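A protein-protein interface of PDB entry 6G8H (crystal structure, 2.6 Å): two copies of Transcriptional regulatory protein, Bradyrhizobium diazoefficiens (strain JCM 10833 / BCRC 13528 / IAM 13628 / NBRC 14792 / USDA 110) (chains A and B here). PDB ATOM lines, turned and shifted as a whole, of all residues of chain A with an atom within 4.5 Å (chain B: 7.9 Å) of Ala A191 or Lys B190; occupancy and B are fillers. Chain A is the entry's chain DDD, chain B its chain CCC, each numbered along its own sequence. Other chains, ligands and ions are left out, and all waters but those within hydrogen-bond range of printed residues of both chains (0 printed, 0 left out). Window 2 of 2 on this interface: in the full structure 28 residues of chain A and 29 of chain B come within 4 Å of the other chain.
Of the 15 printed residues of chain B, 6 touch a printed residue of chain A.
Of the 7 printed residues of chain A, 5 touch a printed residue of chain B.
Hydrophobic or aromatic side chains of chain A within 4 Å of the printed part of chain B: Phe A187, Phe A188 and Ala A191.
Among the printed residues, 11 pairs touch across the chains.
The backbone carbonyl oxygen of Ala B191 sits at hydrogen-bond distance from the side-chain amino group of Lys A190 (2.8 Å).
Among the printed residues, pairs that only touch across the chains: Ala A191 with Lys B190 (2.8 Å), Ala A191 with Phe B187 (3.4 Å), Phe A188 with Phe B187 (3.6 Å), Phe A187 with Phe B188 (3.6 Å), Phe A187 with Ala B191 (3.7 Å), Ala A191 with Ala B191 (3.8 Å), Cys A192 with Phe B187 (3.8 Å), Phe A187 with Cys B192 (3.9 Å), Phe A187 with Leu B156 (3.9 Å) and Lys A190 with Lys B190 (3.98 Å).
Printed residues of chain B within 4 Å of Phe A187: Leu B156, Phe B188, Ala B191 and Cys B192.
Of the printed residues of chain B, Phe A188 touches Phe B187.
Lys B190 touches just these residues of chain A: Lys A190 (3.98 Å) and Ala A191 (2.8 Å).
Of the printed residues of chain A, Ala B191 touches Phe A187, Lys A190 and Ala A191.
The nearest printed residue of chain A that does not touch Lys B190 is Cys A192 (4.9 Å).
The nearest printed residue of chain B that does not touch Phe A188 is Ala B191 (6.1 Å).
The backbone carbonyl oxygen of Phe B188 lies close to the side-chain sulfur of Cys B192, 3.6 Å away.
The backbone carbonyl oxygen (O) of Phe A188 sits close to the side-chain sulfur (SG) of Cys A192 (3.6 Å).
Phe A187 touches Phe B188, and with the chains exchanged Phe A188 touches Phe B187.
Phe A187 touches Ala B191, and with the chains exchanged Ala A191 touches Phe B187.
Lys A190 touches its own counterpart, Lys B190.
Lys A190 touches Ala B191, and with the chains exchanged Ala A191 touches Lys B190.
Positions printed for both chains: 187, 188, 189, 190, 191, 192 and 193.
Of the 11 pairs that touch across the chains among the printed residues, 10 have their exchanged pair printed and touching as well.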
ATOM      1  N   PHE A 187     -12.192  26.858  14.591  1.00  0.00           N
ATOM      2  CA  PHE A 187     -11.378  25.788  15.185  1.00  0.00           C
ATOM      3  C   PHE A 187     -12.243  24.988  16.155  1.00  0.00           C
ATOM      4  O   PHE A 187     -12.177  23.774  16.161  1.00  0.00           O
ATOM      5  CB  PHE A 187     -10.167  26.416  15.861  1.00  0.00           C
ATOM      6  CG  PHE A 187      -9.125  25.423  16.278  1.00  0.00           C
ATOM      7  CD1 PHE A 187      -9.247  24.742  17.483  1.00  0.00           C
ATOM      8  CD2 PHE A 187      -8.030  25.179  15.471  1.00  0.00           C
ATOM      9  CE1 PHE A 187      -8.283  23.821  17.858  1.00  0.00           C
ATOM     10  CE2 PHE A 187      -7.059  24.267  15.862  1.00  0.00           C
ATOM     11  CZ  PHE A 187      -7.184  23.598  17.054  1.00  0.00           C
ATOM     12  N   PHE A 188     -13.038  25.675  16.958  1.00  0.00           N
ATOM     13  CA  PHE A 188     -13.983  25.069  17.914  1.00  0.00           C
ATOM     14  C   PHE A 188     -14.958  24.150  17.173  1.00  0.00           C
ATOM     15  O   PHE A 188     -15.219  23.040  17.634  1.00  0.00           O
ATOM     16  CB  PHE A 188     -14.738  26.159  18.657  1.00  0.00           C
ATOM     17  CG  PHE A 188     -15.660  25.620  19.717  1.00  0.00           C
ATOM     18  CD1 PHE A 188     -15.158  25.161  20.916  1.00  0.00           C
ATOM     19  CD2 PHE A 188     -17.026  25.587  19.512  1.00  0.00           C
ATOM     20  CE1 PHE A 188     -16.016  24.713  21.903  1.00  0.00           C
ATOM     21  CE2 PHE A 188     -17.884  25.136  20.500  1.00  0.00           C
ATOM     22  CZ  PHE A 188     -17.373  24.695  21.693  1.00  0.00           C
ATOM     23  N   LEU A 189     -15.487  24.612  16.055  1.00  0.00           N
ATOM     24  CA  LEU A 189     -16.437  23.832  15.225  1.00  0.00           C
ATOM     25  C   LEU A 189     -15.699  22.650  14.562  1.00  0.00           C
ATOM     26  O   LEU A 189     -16.273  21.548  14.538  1.00  0.00           O
ATOM     27  CB  LEU A 189     -17.116  24.751  14.206  1.00  0.00           C
ATOM     28  CG  LEU A 189     -18.001  25.844  14.827  1.00  0.00           C
ATOM     29  CD1 LEU A 189     -18.663  26.734  13.776  1.00  0.00           C
ATOM     30  CD2 LEU A 189     -19.058  25.236  15.711  1.00  0.00           C
ATOM     31  N   LYS A 190     -14.476  22.826  14.058  1.00  0.00           N
ATOM     32  CA  LYS A 190     -13.706  21.696  13.465  1.00  0.00           C
ATOM     33  C   LYS A 190     -13.634  20.579  14.509  1.00  0.00           C
ATOM     34  O   LYS A 190     -13.703  19.420  14.128  1.00  0.00           O
ATOM     35  CB  LYS A 190     -12.294  22.087  13.002  1.00  0.00           C
ATOM     36  CG  LYS A 190     -12.135  22.863  11.688  1.00  0.00           C
ATOM     37  CD  LYS A 190     -12.302  22.151  10.325  1.00  0.00           C
ATOM     38  CE  LYS A 190     -11.867  20.691  10.257  1.00  0.00           C
ATOM     39  NZ  LYS A 190     -10.443  20.463  10.613  1.00  0.00           N
ATOM     40  N   ALA A 191     -13.565  20.902  15.797  1.00  0.00           N
ATOM     41  CA  ALA A 191     -13.325  19.913  16.876  1.00  0.00           C
ATOM     42  C   ALA A 191     -14.633  19.324  17.426  1.00  0.00           C
ATOM     43  O   ALA A 191     -14.570  18.250  18.015  1.00  0.00           O
ATOM     44  CB  ALA A 191     -12.526  20.560  17.979  1.00  0.00           C
ATOM     45  N   CYS A 192     -15.770  20.007  17.300  1.00  0.00           N
ATOM     46  CA  CYS A 192     -17.014  19.666  18.039  1.00  0.00           C
ATOM     47  C   CYS A 192     -18.199  19.337  17.120  1.00  0.00           C
ATOM     48  O   CYS A 192     -19.151  18.782  17.629  1.00  0.00           O
ATOM     49  CB  CYS A 192     -17.421  20.817  18.948  1.00  0.00           C
ATOM     50  SG  CYS A 192     -16.323  21.010  20.364  1.00  0.00           S
ATOM     51  N   GLN A 193     -18.197  19.737  15.850  1.00  0.00           N
ATOM     52  CA  GLN A 193     -19.285  19.375  14.899  1.00  0.00           C
ATOM     53  C   GLN A 193     -19.198  17.888  14.584  1.00  0.00           C
ATOM     54  O   GLN A 193     -18.107  17.336  14.482  1.00  0.00           O
ATOM     55  CB  GLN A 193     -19.231  20.206  13.619  1.00  0.00           C
ATOM     56  CG  GLN A 193     -19.571  21.667  13.882  1.00  0.00           C
ATOM     57  CD  GLN A 193     -20.144  22.413  12.699  1.00  0.00           C
ATOM     58  OE1 GLN A 193     -19.444  22.770  11.747  1.00  0.00           O
ATOM     59  NE2 GLN A 193     -21.424  22.717  12.798  1.00  0.00           N
ATOM     60  N   LEU B 141      -0.883  16.220  10.485  1.00  0.00           N
ATOM     61  CA  LEU B 141      -1.834  17.305  10.870  1.00  0.00           C
ATOM     62  C   LEU B 141      -2.294  18.022   9.598  1.00  0.00           C
ATOM     63  O   LEU B 141      -1.473  18.115   8.672  1.00  0.00           O
ATOM     64  CB  LEU B 141      -1.149  18.349  11.761  1.00  0.00           C
ATOM     65  CG  LEU B 141      -0.674  17.906  13.139  1.00  0.00           C
ATOM     66  CD1 LEU B 141      -0.046  19.065  13.867  1.00  0.00           C
ATOM     67  CD2 LEU B 141      -1.791  17.356  13.989  1.00  0.00           C
ATOM     68  N   LEU B 156      -5.180  26.368  24.352  1.00  0.00           N
ATOM     69  CA  LEU B 156      -6.015  25.261  24.847  1.00  0.00           C
ATOM     70  C   LEU B 156      -5.384  24.706  26.119  1.00  0.00           C
ATOM     71  O   LEU B 156      -6.081  24.579  27.102  1.00  0.00           O
ATOM     72  CB  LEU B 156      -6.122  24.211  23.755  1.00  0.00           C
ATOM     73  CG  LEU B 156      -7.102  24.569  22.662  1.00  0.00           C
ATOM     74  CD1 LEU B 156      -6.997  23.566  21.535  1.00  0.00           C
ATOM     75  CD2 LEU B 156      -8.510  24.610  23.212  1.00  0.00           C
ATOM     76  N   ALA B 183      -6.322  17.258  27.933  1.00  0.00           N
ATOM     77  CA  ALA B 183      -7.622  17.847  27.520  1.00  0.00           C
ATOM     78  C   ALA B 183      -7.393  18.792  26.329  1.00  0.00           C
ATOM     79  O   ALA B 183      -8.141  18.724  25.328  1.00  0.00           O
ATOM     80  CB  ALA B 183      -8.251  18.557  28.700  1.00  0.00           C
ATOM     81  N   GLY B 184      -6.367  19.629  26.444  1.00  0.00           N
ATOM     82  CA  GLY B 184      -5.975  20.589  25.410  1.00  0.00           C
ATOM     83  C   GLY B 184      -5.502  19.866  24.181  1.00  0.00           C
ATOM     84  O   GLY B 184      -5.887  20.240  23.061  1.00  0.00           O
ATOM     85  N   LEU B 185      -4.718  18.825  24.389  1.00  0.00           N
ATOM     86  CA  LEU B 185      -4.132  18.010  23.296  1.00  0.00           C
ATOM     87  C   LEU B 185      -5.242  17.218  22.578  1.00  0.00           C
ATOM     88  O   LEU B 185      -5.248  17.206  21.352  1.00  0.00           O
ATOM     89  CB  LEU B 185      -3.075  17.103  23.928  1.00  0.00           C
ATOM     90  CG  LEU B 185      -2.416  16.137  22.967  1.00  0.00           C
ATOM     91  CD1 LEU B 185      -1.811  16.892  21.799  1.00  0.00           C
ATOM     92  CD2 LEU B 185      -1.349  15.324  23.688  1.00  0.00           C
ATOM     93  N   LYS B 186      -6.143  16.589  23.330  1.00  0.00           N
ATOM     94  CA  LYS B 186      -7.310  15.829  22.808  1.00  0.00           C
ATOM     95  C   LYS B 186      -8.048  16.742  21.834  1.00  0.00           C
ATOM     96  O   LYS B 186      -8.359  16.325  20.703  1.00  0.00           O
ATOM     97  CB  LYS B 186      -8.219  15.349  23.951  1.00  0.00           C
ATOM     98  CG  LYS B 186      -8.779  13.935  23.778  1.00  0.00           C
ATOM     99  CD  LYS B 186      -9.936  13.709  22.757  1.00  0.00           C
ATOM    100  CE  LYS B 186      -9.621  13.533  21.261  1.00  0.00           C
ATOM    101  NZ  LYS B 186      -8.397  12.761  20.913  1.00  0.00           N
ATOM    102  N   PHE B 187      -8.266  17.988  22.245  1.00  0.00           N
ATOM    103  CA  PHE B 187      -9.139  18.939  21.524  1.00  0.00           C
ATOM    104  C   PHE B 187      -8.428  19.370  20.251  1.00  0.00           C
ATOM    105  O   PHE B 187      -9.042  19.415  19.174  1.00  0.00           O
ATOM    106  CB  PHE B 187      -9.491  20.116  22.419  1.00  0.00           C
ATOM    107  CG  PHE B 187     -10.584  20.999  21.856  1.00  0.00           C
ATOM    108  CD1 PHE B 187     -10.335  21.945  20.855  1.00  0.00           C
ATOM    109  CD2 PHE B 187     -11.866  20.927  22.384  1.00  0.00           C
ATOM    110  CE1 PHE B 187     -11.355  22.733  20.356  1.00  0.00           C
ATOM    111  CE2 PHE B 187     -12.880  21.742  21.891  1.00  0.00           C
ATOM    112  CZ  PHE B 187     -12.618  22.637  20.876  1.00  0.00           C
ATOM    113  N   PHE B 188      -7.147  19.678  20.385  1.00  0.00           N
ATOM    114  CA  PHE B 188      -6.296  20.150  19.274  1.00  0.00           C
ATOM    115  C   PHE B 188      -6.263  19.087  18.178  1.00  0.00           C
ATOM    116  O   PHE B 188      -6.361  19.410  16.995  1.00  0.00           O
ATOM    117  CB  PHE B 188      -4.897  20.461  19.812  1.00  0.00           C
ATOM    118  CG  PHE B 188      -3.965  20.974  18.757  1.00  0.00           C
ATOM    119  CD1 PHE B 188      -4.086  22.259  18.307  1.00  0.00           C
ATOM    120  CD2 PHE B 188      -3.012  20.160  18.183  1.00  0.00           C
ATOM    121  CE1 PHE B 188      -3.265  22.734  17.306  1.00  0.00           C
ATOM    122  CE2 PHE B 188      -2.193  20.633  17.182  1.00  0.00           C
ATOM    123  CZ  PHE B 188      -2.302  21.930  16.767  1.00  0.00           C
ATOM    124  N   LEU B 189      -6.092  17.838  18.575  1.00  0.00           N
ATOM    125  CA  LEU B 189      -6.028  16.693  17.638  1.00  0.00           C
ATOM    126  C   LEU B 189      -7.414  16.439  17.031  1.00  0.00           C
ATOM    127  O   LEU B 189      -7.456  16.153  15.838  1.00  0.00           O
ATOM    128  CB  LEU B 189      -5.459  15.482  18.389  1.00  0.00           C
ATOM    129  CG  LEU B 189      -3.985  15.626  18.793  1.00  0.00           C
ATOM    130  CD1 LEU B 189      -3.456  14.355  19.434  1.00  0.00           C
ATOM    131  CD2 LEU B 189      -3.114  16.004  17.596  1.00  0.00           C
ATOM    132  N   LYS B 190      -8.511  16.550  17.784  1.00  0.00           N
ATOM    133  CA  LYS B 190      -9.870  16.383  17.188  1.00  0.00           C
ATOM    134  C   LYS B 190     -10.002  17.368  16.012  1.00  0.00           C
ATOM    135  O   LYS B 190     -10.650  17.040  15.032  1.00  0.00           O
ATOM    136  CB  LYS B 190     -10.995  16.565  18.216  1.00  0.00           C
ATOM    137  CG  LYS B 190     -11.813  15.310  18.498  1.00  0.00           C
ATOM    138  CD  LYS B 190     -13.279  15.542  18.888  1.00  0.00           C
ATOM    139  CE  LYS B 190     -13.527  16.579  19.981  1.00  0.00           C
ATOM    140  NZ  LYS B 190     -12.804  16.302  21.256  1.00  0.00           N
ATOM    141  N   ALA B 191      -9.373  18.536  16.084  1.00  0.00           N
ATOM    142  CA  ALA B 191      -9.553  19.612  15.091  1.00  0.00           C
ATOM    143  C   ALA B 191      -8.540  19.503  13.938  1.00  0.00           C
ATOM    144  O   ALA B 191      -8.822  20.081  12.879  1.00  0.00           O
ATOM    145  CB  ALA B 191      -9.452  20.939  15.796  1.00  0.00           C
ATOM    146  N   CYS B 192      -7.395  18.853  14.118  1.00  0.00           N
ATOM    147  CA  CYS B 192      -6.252  18.937  13.171  1.00  0.00           C
ATOM    148  C   CYS B 192      -5.840  17.590  12.573  1.00  0.00           C
ATOM    149  O   CYS B 192      -5.164  17.627  11.550  1.00  0.00           O
ATOM    150  CB  CYS B 192      -5.036  19.556  13.848  1.00  0.00           C
ATOM    151  SG  CYS B 192      -5.225  21.321  14.171  1.00  0.00           S
ATOM    152  N   GLN B 193      -6.160  16.458  13.200  1.00  0.00           N
ATOM    153  CA  GLN B 193      -5.866  15.114  12.633  1.00  0.00           C
ATOM    154  C   GLN B 193      -6.715  14.874  11.395  1.00  0.00           C
ATOM    155  O   GLN B 193      -7.877  15.267  11.361  1.00  0.00           O
ATOM    156  CB  GLN B 193      -6.132  13.997  13.633  1.00  0.00           C
ATOM    157  CG  GLN B 193      -5.118  14.000  14.760  1.00  0.00           C
ATOM    158  CD  GLN B 193      -4.984  12.668  15.448  1.00  0.00           C
ATOM    159  OE1 GLN B 193      -5.858  12.227  16.200  1.00  0.00           O
ATOM    160  NE2 GLN B 193      -3.819  12.084  15.266  1.00  0.00           N
ATOM    161  N   PRO B 194      -6.141  14.239  10.346  1.00  0.00           N
ATOM    162  CA  PRO B 194      -6.935  13.753   9.212  1.00  0.00           C
ATOM    163  C   PRO B 194      -8.049  12.787   9.661  1.00  0.00           C
ATOM    164  O   PRO B 194      -7.749  11.898  10.448  1.00  0.00           O
ATOM    165  CB  PRO B 194      -5.871  13.071   8.333  1.00  0.00           C
ATOM    166  CG  PRO B 194      -4.603  13.829   8.665  1.00  0.00           C
ATOM    167  CD  PRO B 194      -4.691  14.022  10.163  1.00  0.00           C
ATOM    168  N   ARG B 195      -9.285  13.033   9.188  1.00  0.00           N
ATOM    169  CA  ARG B 195     -10.569  12.442   9.664  1.00  0.00           C
ATOM    170  C   ARG B 195     -11.083  11.440   8.614  1.00  0.00           C
ATOM    171  O   ARG B 195     -10.509  10.380   8.342  1.00  0.00           O
ATOM    172  CB  ARG B 195     -11.578  13.571   9.946  1.00  0.00           C
